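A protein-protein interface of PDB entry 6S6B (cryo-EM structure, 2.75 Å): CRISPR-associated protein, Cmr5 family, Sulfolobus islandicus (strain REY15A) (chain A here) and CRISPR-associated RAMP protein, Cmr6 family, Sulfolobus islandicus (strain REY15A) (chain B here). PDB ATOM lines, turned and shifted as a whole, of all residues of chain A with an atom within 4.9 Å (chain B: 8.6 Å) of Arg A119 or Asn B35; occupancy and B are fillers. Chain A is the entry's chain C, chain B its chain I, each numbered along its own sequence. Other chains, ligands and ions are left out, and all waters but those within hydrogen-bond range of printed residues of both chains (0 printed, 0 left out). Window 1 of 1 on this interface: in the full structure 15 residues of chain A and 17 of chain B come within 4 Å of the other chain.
The guanidinium group (NH1) of Arg A119 sits at hydrogen-bond distance from the side-chain amide oxygen (OD1) of Asn B35 (3.2 Å).
The side-chain hydroxyl (OG) of Ser B41 sits at hydrogen-bond distance from the side-chain amino group (NZ) of Lys A117 (2.7 Å).
OE2 of Glu B38 is in salt-bridge range of NH2 of Arg A119 (3.9 Å).
OH of Tyr B46 sits at hydrogen-bond distance from O of Phe B39 (3.5 Å).
The side-chain amide oxygen (OD1) of Asn B34 lies within hydrogen-bond range of the guanidinium group (NH2) of Arg B73, at 3.4 Å.
The backbone carbonyl oxygen (O) of Glu B38 is in hydrogen-bond range of the side-chain hydroxyl (OG) of Ser B41.
The backbone carbonyl oxygen (O) of Ala A112 is in hydrogen-bond range of the guanidinium group (NE) of Arg A119 (3.2 Å).
O of Ile B31 lies within hydrogen-bond range of ND2 of Asn B35 (2.5 Å).
The side-chain amide nitrogen (ND2) of Asn B34 lies within hydrogen-bond range of the backbone carbonyl oxygen (O) of Leu B135 (3.4 Å).
Phe A51 touches Ile B31 (CD2 to CG2, 3.98 Å).
Phe A51 touches Asn B34.
Phe A51 touches Asn B35 (CD1 to OD1, 3.6 Å).
Gly B37 touches Glu A116 (O to OE1, 3.8 Å).
Glu A116 touches Glu B38 (O to CG, 3.5 Å).
Glu A116 touches Ser B41 (OE1 to CB, 3.6 Å).
Ile B3 touches Leu A120.
Glu B38 touches Leu A120 (CB to CD2, 3.5 Å).
CD1 of Ile A123 touches ND2 of Asn B35 (3.9 Å).
CD1 of Ile A123 touches CE1 of Phe B39 (3.9 Å).
Arg A119 touches two residues of chain B.
Of the printed residues of chain B, Ile A123 touches Asn B35 (3.9 Å) and Phe B39 (3.9 Å).
Printed residues of chain A within 4 Å of Asn B35: Phe A51, Arg A119 and Ile A123.
Of the printed residues of chain A, Gly B37 touches Glu A116.
Phe B76 touches none of the printed residues of chain A.
The nearest printed residue of chain B that does not touch Leu A120 is Ser B41 (5.3 Å).
Of the 23 printed residues of chain B, 9 touch a printed residue of chain A.
Printed residues of chain A that touch a printed residue of chain B: Phe A51, Glu A116, Lys A117, Arg A119, Leu A120 and Ile A123.
Hydrophobic or aromatic side chains of chain A within 4 Å of the printed part of chain B: Phe A51, Leu A120 and Ile A123.
Among the printed residues, 15 pairs touch across the chains.
Among the printed residues, Asp or Glu carboxylates within 4 Å of a Lys or Arg side-chain nitrogen of the other chain: Arg A119 with Glu B38.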
ATOM      1  N   PHE A  51      20.548  15.311  22.230  1.00  0.00           N
ATOM      2  CA  PHE A  51      21.228  15.854  23.396  1.00  0.00           C
ATOM      3  C   PHE A  51      20.271  16.074  24.551  1.00  0.00           C
ATOM      4  O   PHE A  51      20.692  16.068  25.710  1.00  0.00           O
ATOM      5  CB  PHE A  51      21.940  17.150  23.026  1.00  0.00           C
ATOM      6  CG  PHE A  51      23.093  16.940  22.112  1.00  0.00           C
ATOM      7  CD1 PHE A  51      24.234  16.310  22.561  1.00  0.00           C
ATOM      8  CD2 PHE A  51      23.027  17.338  20.796  1.00  0.00           C
ATOM      9  CE1 PHE A  51      25.293  16.097  21.721  1.00  0.00           C
ATOM     10  CE2 PHE A  51      24.084  17.129  19.950  1.00  0.00           C
ATOM     11  CZ  PHE A  51      25.218  16.506  20.415  1.00  0.00           C
ATOM     12  N   ILE A  54      20.635  12.872  26.372  1.00  0.00           N
ATOM     13  CA  ILE A  54      21.863  12.777  27.153  1.00  0.00           C
ATOM     14  C   ILE A  54      21.758  13.604  28.424  1.00  0.00           C
ATOM     15  O   ILE A  54      22.329  13.240  29.458  1.00  0.00           O
ATOM     16  CB  ILE A  54      23.077  13.208  26.315  1.00  0.00           C
ATOM     17  CG1 ILE A  54      23.067  12.513  24.961  1.00  0.00           C
ATOM     18  CG2 ILE A  54      24.356  12.880  27.043  1.00  0.00           C
ATOM     19  CD1 ILE A  54      24.363  12.635  24.215  1.00  0.00           C
ATOM     20  N   ALA A 112      32.864  11.290  23.364  1.00  0.00           N
ATOM     21  CA  ALA A 112      32.001  12.462  23.381  1.00  0.00           C
ATOM     22  C   ALA A 112      31.211  12.533  24.678  1.00  0.00           C
ATOM     23  O   ALA A 112      31.233  13.552  25.376  1.00  0.00           O
ATOM     24  CB  ALA A 112      31.063  12.438  22.176  1.00  0.00           C
ATOM     25  N   LEU A 113      30.514  11.453  25.023  1.00  0.00           N
ATOM     26  CA  LEU A 113      29.724  11.437  26.247  1.00  0.00           C
ATOM     27  C   LEU A 113      30.596  11.584  27.482  1.00  0.00           C
ATOM     28  O   LEU A 113      30.156  12.149  28.488  1.00  0.00           O
ATOM     29  CB  LEU A 113      28.918  10.145  26.325  1.00  0.00           C
ATOM     30  CG  LEU A 113      27.504  10.157  25.751  1.00  0.00           C
ATOM     31  CD1 LEU A 113      27.503  10.612  24.310  1.00  0.00           C
ATOM     32  CD2 LEU A 113      26.914   8.776  25.854  1.00  0.00           C
ATOM     33  N   CYS A 115      34.096  12.908  27.913  1.00  0.00           N
ATOM     34  CA  CYS A 115      34.815  14.162  28.070  1.00  0.00           C
ATOM     35  C   CYS A 115      34.105  15.295  27.342  1.00  0.00           C
ATOM     36  O   CYS A 115      33.539  15.112  26.263  1.00  0.00           O
ATOM     37  CB  CYS A 115      36.247  14.021  27.558  1.00  0.00           C
ATOM     38  SG  CYS A 115      37.268  12.935  28.568  1.00  0.00           S
ATOM     39  N   GLU A 116      34.154  16.481  27.946  1.00  0.00           N
ATOM     40  CA  GLU A 116      33.388  17.617  27.454  1.00  0.00           C
ATOM     41  C   GLU A 116      33.959  18.225  26.185  1.00  0.00           C
ATOM     42  O   GLU A 116      33.220  18.882  25.445  1.00  0.00           O
ATOM     43  CB  GLU A 116      33.311  18.697  28.531  1.00  0.00           C
ATOM     44  CG  GLU A 116      34.665  19.103  29.072  1.00  0.00           C
ATOM     45  CD  GLU A 116      34.656  20.479  29.704  1.00  0.00           C
ATOM     46  OE1 GLU A 116      33.600  21.143  29.666  1.00  0.00           O
ATOM     47  OE2 GLU A 116      35.704  20.896  30.239  1.00  0.00           O
ATOM     48  N   LYS A 117      35.251  18.041  25.919  1.00  0.00           N
ATOM     49  CA  LYS A 117      35.869  18.741  24.800  1.00  0.00           C
ATOM     50  C   LYS A 117      35.388  18.185  23.468  1.00  0.00           C
ATOM     51  O   LYS A 117      35.000  18.942  22.572  1.00  0.00           O
ATOM     52  CB  LYS A 117      37.392  18.664  24.906  1.00  0.00           C
ATOM     53  CG  LYS A 117      37.981  19.545  26.004  1.00  0.00           C
ATOM     54  CD  LYS A 117      37.195  20.843  26.175  1.00  0.00           C
ATOM     55  CE  LYS A 117      37.477  21.840  25.053  1.00  0.00           C
ATOM     56  NZ  LYS A 117      36.715  23.107  25.230  1.00  0.00           N
ATOM     57  N   THR A 118      35.398  16.865  23.320  1.00  0.00           N
ATOM     58  CA  THR A 118      34.921  16.256  22.090  1.00  0.00           C
ATOM     59  C   THR A 118      33.405  16.230  21.998  1.00  0.00           C
ATOM     60  O   THR A 118      32.872  15.844  20.953  1.00  0.00           O
ATOM     61  CB  THR A 118      35.465  14.836  21.962  1.00  0.00           C
ATOM     62  OG1 THR A 118      34.716  13.964  22.811  1.00  0.00           O
ATOM     63  CG2 THR A 118      36.922  14.796  22.380  1.00  0.00           C
ATOM     64  N   ARG A 119      32.699  16.627  23.056  1.00  0.00           N
ATOM     65  CA  ARG A 119      31.247  16.712  22.976  1.00  0.00           C
ATOM     66  C   ARG A 119      30.814  17.750  21.951  1.00  0.00           C
ATOM     67  O   ARG A 119      29.863  17.526  21.197  1.00  0.00           O
ATOM     68  CB  ARG A 119      30.663  17.039  24.348  1.00  0.00           C
ATOM     69  CG  ARG A 119      29.171  17.282  24.331  1.00  0.00           C
ATOM     70  CD  ARG A 119      28.405  15.980  24.260  1.00  0.00           C
ATOM     71  NE  ARG A 119      28.475  15.249  25.518  1.00  0.00           N
ATOM     72  CZ  ARG A 119      27.640  15.434  26.532  1.00  0.00           C
ATOM     73  NH1 ARG A 119      26.667  16.326  26.434  1.00  0.00           N
ATOM     74  NH2 ARG A 119      27.776  14.728  27.643  1.00  0.00           N
ATOM     75  N   LEU A 120      31.500  18.893  21.908  1.00  0.00           N
ATOM     76  CA  LEU A 120      31.156  19.908  20.920  1.00  0.00           C
ATOM     77  C   LEU A 120      31.458  19.416  19.516  1.00  0.00           C
ATOM     78  O   LEU A 120      30.720  19.719  18.572  1.00  0.00           O
ATOM     79  CB  LEU A 120      31.919  21.204  21.188  1.00  0.00           C
ATOM     80  CG  LEU A 120      31.445  22.150  22.290  1.00  0.00           C
ATOM     81  CD1 LEU A 120      30.006  22.578  22.080  1.00  0.00           C
ATOM     82  CD2 LEU A 120      31.645  21.533  23.656  1.00  0.00           C
ATOM     83  N   ASP A 121      32.545  18.663  19.358  1.00  0.00           N
ATOM     84  CA  ASP A 121      32.869  18.106  18.053  1.00  0.00           C
ATOM     85  C   ASP A 121      31.815  17.107  17.605  1.00  0.00           C
ATOM     86  O   ASP A 121      31.563  16.964  16.405  1.00  0.00           O
ATOM     87  CB  ASP A 121      34.246  17.450  18.095  1.00  0.00           C
ATOM     88  CG  ASP A 121      34.818  17.217  16.715  1.00  0.00           C
ATOM     89  OD1 ASP A 121      35.278  16.089  16.442  1.00  0.00           O
ATOM     90  OD2 ASP A 121      34.817  18.167  15.903  1.00  0.00           O
ATOM     91  N   LEU A 122      31.189  16.412  18.555  1.00  0.00           N
ATOM     92  CA  LEU A 122      30.084  15.525  18.216  1.00  0.00           C
ATOM     93  C   LEU A 122      28.911  16.307  17.647  1.00  0.00           C
ATOM     94  O   LEU A 122      28.241  15.844  16.718  1.00  0.00           O
ATOM     95  CB  LEU A 122      29.652  14.734  19.444  1.00  0.00           C
ATOM     96  CG  LEU A 122      28.285  14.065  19.345  1.00  0.00           C
ATOM     97  CD1 LEU A 122      28.323  12.953  18.318  1.00  0.00           C
ATOM     98  CD2 LEU A 122      27.854  13.536  20.694  1.00  0.00           C
ATOM     99  N   ILE A 123      28.646  17.496  18.189  1.00  0.00           N
ATOM    100  CA  ILE A 123      27.557  18.317  17.671  1.00  0.00           C
ATOM    101  C   ILE A 123      27.782  18.646  16.206  1.00  0.00           C
ATOM    102  O   ILE A 123      26.827  18.847  15.450  1.00  0.00           O
ATOM    103  CB  ILE A 123      27.405  19.593  18.518  1.00  0.00           C
ATOM    104  CG1 ILE A 123      27.293  19.231  19.997  1.00  0.00           C
ATOM    105  CG2 ILE A 123      26.195  20.393  18.072  1.00  0.00           C
ATOM    106  CD1 ILE A 123      26.813  20.360  20.868  1.00  0.00           C
ATOM    107  N   ILE B   3      28.552  24.704  14.699  1.00  0.00           N
ATOM    108  CA  ILE B   3      28.645  25.153  16.081  1.00  0.00           C
ATOM    109  C   ILE B   3      28.820  26.663  16.138  1.00  0.00           C
ATOM    110  O   ILE B   3      28.373  27.312  17.089  1.00  0.00           O
ATOM    111  CB  ILE B   3      29.788  24.419  16.800  1.00  0.00           C
ATOM    112  CG1 ILE B   3      29.869  24.855  18.260  1.00  0.00           C
ATOM    113  CG2 ILE B   3      31.110  24.654  16.082  1.00  0.00           C
ATOM    114  CD1 ILE B   3      30.906  24.112  19.044  1.00  0.00           C
ATOM    115  N   LEU B   6      25.171  27.974  16.254  1.00  0.00           N
ATOM    116  CA  LEU B   6      24.338  27.826  17.440  1.00  0.00           C
ATOM    117  C   LEU B   6      24.703  28.846  18.506  1.00  0.00           C
ATOM    118  O   LEU B   6      23.819  29.416  19.151  1.00  0.00           O
ATOM    119  CB  LEU B   6      24.467  26.413  18.000  1.00  0.00           C
ATOM    120  CG  LEU B   6      23.864  25.304  17.147  1.00  0.00           C
ATOM    121  CD1 LEU B   6      24.295  23.952  17.663  1.00  0.00           C
ATOM    122  CD2 LEU B   6      22.362  25.417  17.147  1.00  0.00           C
ATOM    123  N   LEU B  28      16.926  24.801  18.424  1.00  0.00           N
ATOM    124  CA  LEU B  28      18.372  24.965  18.358  1.00  0.00           C
ATOM    125  C   LEU B  28      18.932  25.430  19.692  1.00  0.00           C
ATOM    126  O   LEU B  28      20.017  25.000  20.099  1.00  0.00           O
ATOM    127  CB  LEU B  28      18.739  25.945  17.250  1.00  0.00           C
ATOM    128  CG  LEU B  28      18.471  25.426  15.840  1.00  0.00           C
ATOM    129  CD1 LEU B  28      18.987  26.396  14.815  1.00  0.00           C
ATOM    130  CD2 LEU B  28      19.100  24.071  15.652  1.00  0.00           C
ATOM    131  N   THR B  29      18.209  26.311  20.383  1.00  0.00           N
ATOM    132  CA  THR B  29      18.630  26.738  21.712  1.00  0.00           C
ATOM    133  C   THR B  29      18.774  25.551  22.649  1.00  0.00           C
ATOM    134  O   THR B  29      19.718  25.487  23.444  1.00  0.00           O
ATOM    135  CB  THR B  29      17.626  27.736  22.275  1.00  0.00           C
ATOM    136  OG1 THR B  29      17.598  28.899  21.444  1.00  0.00           O
ATOM    137  CG2 THR B  29      18.007  28.129  23.678  1.00  0.00           C
ATOM    138  N   SER B  30      17.852  24.594  22.562  1.00  0.00           N
ATOM    139  CA  SER B  30      17.903  23.419  23.418  1.00  0.00           C
ATOM    140  C   SER B  30      19.203  22.644  23.272  1.00  0.00           C
ATOM    141  O   SER B  30      19.563  21.890  24.180  1.00  0.00           O
ATOM    142  CB  SER B  30      16.721  22.507  23.114  1.00  0.00           C
ATOM    143  OG  SER B  30      16.948  21.763  21.936  1.00  0.00           O
ATOM    144  N   ILE B  31      19.916  22.804  22.157  1.00  0.00           N
ATOM    145  CA  ILE B  31      21.218  22.161  22.044  1.00  0.00           C
ATOM    146  C   ILE B  31      22.225  22.857  22.940  1.00  0.00           C
ATOM    147  O   ILE B  31      23.168  22.229  23.433  1.00  0.00           O
ATOM    148  CB  ILE B  31      21.690  22.140  20.581  1.00  0.00           C
ATOM    149  CG1 ILE B  31      20.595  21.586  19.678  1.00  0.00           C
ATOM    150  CG2 ILE B  31      22.939  21.301  20.439  1.00  0.00           C
ATOM    151  CD1 ILE B  31      20.969  21.571  18.225  1.00  0.00           C
ATOM    152  N   VAL B  32      22.046  24.155  23.176  1.00  0.00           N
ATOM    153  CA  VAL B  32      22.935  24.870  24.081  1.00  0.00           C
ATOM    154  C   VAL B  32      22.510  24.662  25.522  1.00  0.00           C
ATOM    155  O   VAL B  32      23.348  24.450  26.402  1.00  0.00           O
ATOM    156  CB  VAL B  32      22.978  26.360  23.718  1.00  0.00           C
ATOM    157  CG1 VAL B  32      24.060  27.049  24.511  1.00  0.00           C
ATOM    158  CG2 VAL B  32      23.206  26.530  22.238  1.00  0.00           C
ATOM    159  N   TYR B  33      21.204  24.717  25.787  1.00  0.00           N
ATOM    160  CA  TYR B  33      20.713  24.505  27.141  1.00  0.00           C
ATOM    161  C   TYR B  33      21.051  23.115  27.652  1.00  0.00           C
ATOM    162  O   TYR B  33      21.223  22.922  28.859  1.00  0.00           O
ATOM    163  CB  TYR B  33      19.207  24.732  27.187  1.00  0.00           C
ATOM    164  CG  TYR B  33      18.555  24.254  28.455  1.00  0.00           C
ATOM    165  CD1 TYR B  33      18.741  24.929  29.648  1.00  0.00           C
ATOM    166  CD2 TYR B  33      17.753  23.128  28.460  1.00  0.00           C
ATOM    167  CE1 TYR B  33      18.149  24.495  30.810  1.00  0.00           C
ATOM    168  CE2 TYR B  33      17.160  22.686  29.616  1.00  0.00           C
ATOM    169  CZ  TYR B  33      17.359  23.375  30.786  1.00  0.00           C
ATOM    170  OH  TYR B  33      16.763  22.936  31.942  1.00  0.00           O
ATOM    171  N   ASN B  34      21.152  22.137  26.760  1.00  0.00           N
ATOM    172  CA  ASN B  34      21.458  20.777  27.170  1.00  0.00           C
ATOM    173  C   ASN B  34      22.949  20.492  27.208  1.00  0.00           C
ATOM    174  O   ASN B  34      23.372  19.580  27.922  1.00  0.00           O
ATOM    175  CB  ASN B  34      20.772  19.782  26.237  1.00  0.00           C
ATOM    176  CG  ASN B  34      19.280  19.738  26.445  1.00  0.00           C
ATOM    177  OD1 ASN B  34      18.804  19.346  27.504  1.00  0.00           O
ATOM    178  ND2 ASN B  34      18.531  20.146  25.435  1.00  0.00           N
ATOM    179  N   ASN B  35      23.748  21.242  26.457  1.00  0.00           N
ATOM    180  CA  ASN B  35      25.199  21.195  26.555  1.00  0.00           C
ATOM    181  C   ASN B  35      25.741  22.440  27.238  1.00  0.00           C
ATOM    182  O   ASN B  35      26.817  22.929  26.891  1.00  0.00           O
ATOM    183  CB  ASN B  35      25.829  21.036  25.177  1.00  0.00           C
ATOM    184  CG  ASN B  35      25.319  19.827  24.450  1.00  0.00           C
ATOM    185  OD1 ASN B  35      25.896  18.747  24.540  1.00  0.00           O
ATOM    186  ND2 ASN B  35      24.228  19.995  23.719  1.00  0.00           N
ATOM    187  N   PHE B  36      24.988  22.968  28.203  1.00  0.00           N
ATOM    188  CA  PHE B  36      25.346  24.234  28.830  1.00  0.00           C
ATOM    189  C   PHE B  36      26.726  24.167  29.464  1.00  0.00           C
ATOM    190  O   PHE B  36      27.544  25.076  29.291  1.00  0.00           O
ATOM    191  CB  PHE B  36      24.297  24.608  29.868  1.00  0.00           C
ATOM    192  CG  PHE B  36      24.500  25.956  30.463  1.00  0.00           C
ATOM    193  CD1 PHE B  36      24.081  27.086  29.797  1.00  0.00           C
ATOM    194  CD2 PHE B  36      25.110  26.097  31.690  1.00  0.00           C
ATOM    195  CE1 PHE B  36      24.264  28.328  30.343  1.00  0.00           C
ATOM    196  CE2 PHE B  36      25.295  27.335  32.237  1.00  0.00           C
ATOM    197  CZ  PHE B  36      24.871  28.452  31.564  1.00  0.00           C
ATOM    198  N   GLY B  37      27.003  23.100  30.209  1.00  0.00           N
ATOM    199  CA  GLY B  37      28.326  22.945  30.781  1.00  0.00           C
ATOM    200  C   GLY B  37      29.416  22.928  29.733  1.00  0.00           C
ATOM    201  O   GLY B  37      30.521  23.419  29.970  1.00  0.00           O
ATOM    202  N   GLU B  38      29.118  22.381  28.556  1.00  0.00           N
ATOM    203  CA  GLU B  38      30.123  22.257  27.511  1.00  0.00           C
ATOM    204  C   GLU B  38      30.338  23.570  26.775  1.00  0.00           C
ATOM    205  O   GLU B  38      31.479  23.941  26.486  1.00  0.00           O
ATOM    206  CB  GLU B  38      29.715  21.157  26.535  1.00  0.00           C
ATOM    207  CG  GLU B  38      30.191  19.777  26.930  1.00  0.00           C
ATOM    208  CD  GLU B  38      29.369  19.164  28.044  1.00  0.00           C
ATOM    209  OE1 GLU B  38      28.387  19.795  28.484  1.00  0.00           O
ATOM    210  OE2 GLU B  38      29.705  18.045  28.480  1.00  0.00           O
ATOM    211  N   PHE B  39      29.262  24.287  26.462  1.00  0.00           N
ATOM    212  CA  PHE B  39      29.385  25.563  25.773  1.00  0.00           C
ATOM    213  C   PHE B  39      30.056  26.632  26.617  1.00  0.00           C
ATOM    214  O   PHE B  39      30.222  27.757  26.138  1.00  0.00           O
ATOM    215  CB  PHE B  39      28.011  26.054  25.333  1.00  0.00           C
ATOM    216  CG  PHE B  39      27.577  25.523  24.005  1.00  0.00           C
ATOM    217  CD1 PHE B  39      26.944  24.300  23.908  1.00  0.00           C
ATOM    218  CD2 PHE B  39      27.800  26.246  22.851  1.00  0.00           C
ATOM    219  CE1 PHE B  39      26.542  23.811  22.691  1.00  0.00           C
ATOM    220  CE2 PHE B  39      27.398  25.758  21.632  1.00  0.00           C
ATOM    221  CZ  PHE B  39      26.769  24.538  21.552  1.00  0.00           C
ATOM    222  N   LEU B  40      30.438  26.318  27.850  1.00  0.00           N
ATOM    223  CA  LEU B  40      31.052  27.285  28.742  1.00  0.00           C
ATOM    224  C   LEU B  40      32.540  27.062  28.954  1.00  0.00           C
ATOM    225  O   LEU B  40      33.183  27.902  29.588  1.00  0.00           O
ATOM    226  CB  LEU B  40      30.356  27.260  30.106  1.00  0.00           C
ATOM    227  CG  LEU B  40      28.967  27.880  30.215  1.00  0.00           C
ATOM    228  CD1 LEU B  40      28.642  28.146  31.666  1.00  0.00           C
ATOM    229  CD2 LEU B  40      28.878  29.157  29.397  1.00  0.00           C
ATOM    230  N   SER B  41      33.103  25.962  28.456  1.00  0.00           N
ATOM    231  CA  SER B  41      34.448  25.581  28.866  1.00  0.00           C
ATOM    232  C   SER B  41      35.498  26.614  28.472  1.00  0.00           C
ATOM    233  O   SER B  41      36.046  27.306  29.335  1.00  0.00           O
ATOM    234  CB  SER B  41      34.811  24.230  28.258  1.00  0.00           C
ATOM    235  OG  SER B  41      34.883  24.321  26.847  1.00  0.00           O
ATOM    236  N   ASN B  43      34.850  28.389  25.132  1.00  0.00           N
ATOM    237  CA  ASN B  43      34.268  28.643  23.815  1.00  0.00           C
ATOM    238  C   ASN B  43      34.114  30.147  23.613  1.00  0.00           C
ATOM    239  O   ASN B  43      33.028  30.722  23.695  1.00  0.00           O
ATOM    240  CB  ASN B  43      32.954  27.892  23.672  1.00  0.00           C
ATOM    241  CG  ASN B  43      33.114  26.417  23.947  1.00  0.00           C
ATOM    242  OD1 ASN B  43      33.419  26.010  25.070  1.00  0.00           O
ATOM    243  ND2 ASN B  43      32.929  25.603  22.918  1.00  0.00           N
ATOM    244  N   TYR B  46      32.955  34.946  21.055  1.00  0.00           N
ATOM    245  CA  TYR B  46      31.596  35.399  21.282  1.00  0.00           C
ATOM    246  C   TYR B  46      31.541  36.913  21.146  1.00  0.00           C
ATOM    247  O   TYR B  46      32.454  37.618  21.583  1.00  0.00           O
ATOM    248  CB  TYR B  46      31.115  34.980  22.669  1.00  0.00           C
ATOM    249  CG  TYR B  46      30.755  33.522  22.800  1.00  0.00           C
ATOM    250  CD1 TYR B  46      30.364  32.997  24.021  1.00  0.00           C
ATOM    251  CD2 TYR B  46      30.804  32.670  21.707  1.00  0.00           C
ATOM    252  CE1 TYR B  46      30.036  31.672  24.154  1.00  0.00           C
ATOM    253  CE2 TYR B  46      30.477  31.337  21.832  1.00  0.00           C
ATOM    254  CZ  TYR B  46      30.091  30.845  23.058  1.00  0.00           C
ATOM    255  OH  TYR B  46      29.763  29.517  23.193  1.00  0.00           O
ATOM    256  N   LEU B  52      26.285  34.417  26.552  1.00  0.00           N
ATOM    257  CA  LEU B  52      26.938  33.347  27.290  1.00  0.00           C
ATOM    258  C   LEU B  52      28.134  33.823  28.098  1.00  0.00           C
ATOM    259  O   LEU B  52      28.563  33.110  29.010  1.00  0.00           O
ATOM    260  CB  LEU B  52      27.383  32.230  26.342  1.00  0.00           C
ATOM    261  CG  LEU B  52      26.385  31.098  26.095  1.00  0.00           C
ATOM    262  CD1 LEU B  52      26.988  30.053  25.183  1.00  0.00           C
ATOM    263  CD2 LEU B  52      25.957  30.473  27.402  1.00  0.00           C
ATOM    264  N   VAL B  69      27.687  24.973  37.820  1.00  0.00           N
ATOM    265  CA  VAL B  69      27.091  24.979  36.490  1.00  0.00           C
ATOM    266  C   VAL B  69      25.593  24.724  36.559  1.00  0.00           C
ATOM    267  O   VAL B  69      24.807  25.428  35.916  1.00  0.00           O
ATOM    268  CB  VAL B  69      27.793  23.958  35.581  1.00  0.00           C
ATOM    269  CG1 VAL B  69      27.090  23.883  34.250  1.00  0.00           C
ATOM    270  CG2 VAL B  69      29.238  24.350  35.384  1.00  0.00           C
ATOM    271  N   ARG B  73      22.661  26.845  34.895  1.00  0.00           N
ATOM    272  CA  ARG B  73      21.735  26.336  33.895  1.00  0.00           C
ATOM    273  C   ARG B  73      20.298  26.676  34.257  1.00  0.00           C
ATOM    274  O   ARG B  73      19.492  26.999  33.380  1.00  0.00           O
ATOM    275  CB  ARG B  73      21.918  24.831  33.744  1.00  0.00           C
ATOM    276  CG  ARG B  73      21.280  24.246  32.509  1.00  0.00           C
ATOM    277  CD  ARG B  73      21.555  22.762  32.429  1.00  0.00           C
ATOM    278  NE  ARG B  73      20.701  22.099  31.456  1.00  0.00           N
ATOM    279  CZ  ARG B  73      20.250  20.859  31.593  1.00  0.00           C
ATOM    280  NH1 ARG B  73      20.573  20.156  32.665  1.00  0.00           N
ATOM    281  NH2 ARG B  73      19.478  20.326  30.662  1.00  0.00           N
ATOM    282  N   PHE B  76      19.932  30.158  33.227  1.00  0.00           N
ATOM    283  CA  PHE B  76      19.889  30.251  31.774  1.00  0.00           C
ATOM    284  C   PHE B  76      18.511  29.891  31.241  1.00  0.00           C
ATOM    285  O   PHE B  76      18.003  30.547  30.326  1.00  0.00           O
ATOM    286  CB  PHE B  76      20.956  29.348  31.163  1.00  0.00           C
ATOM    287  CG  PHE B  76      20.972  29.372  29.672  1.00  0.00           C
ATOM    288  CD1 PHE B  76      21.106  30.562  28.993  1.00  0.00           C
ATOM    289  CD2 PHE B  76      20.843  28.206  28.946  1.00  0.00           C
ATOM    290  CE1 PHE B  76      21.113  30.589  27.622  1.00  0.00           C
ATOM    291  CE2 PHE B  76      20.852  28.229  27.574  1.00  0.00           C
ATOM    292  CZ  PHE B  76      20.987  29.420  26.912  1.00  0.00           C
ATOM    293  N   LEU B 135      12.048  20.437  24.806  1.00  0.00           N
ATOM    294  CA  LEU B 135      13.436  20.087  25.050  1.00  0.00           C
ATOM    295  C   LEU B 135      14.132  21.052  25.992  1.00  0.00           C
ATOM    296  O   LEU B 135      15.288  20.814  26.349  1.00  0.00           O
ATOM    297  CB  LEU B 135      14.189  20.020  23.726  1.00  0.00           C
ATOM    298  CG  LEU B 135      13.555  19.135  22.662  1.00  0.00           C
ATOM    299  CD1 LEU B 135      14.284  19.319  21.363  1.00  0.00           C
ATOM    300  CD2 LEU B 135      13.586  17.688  23.083  1.00  0.00           C
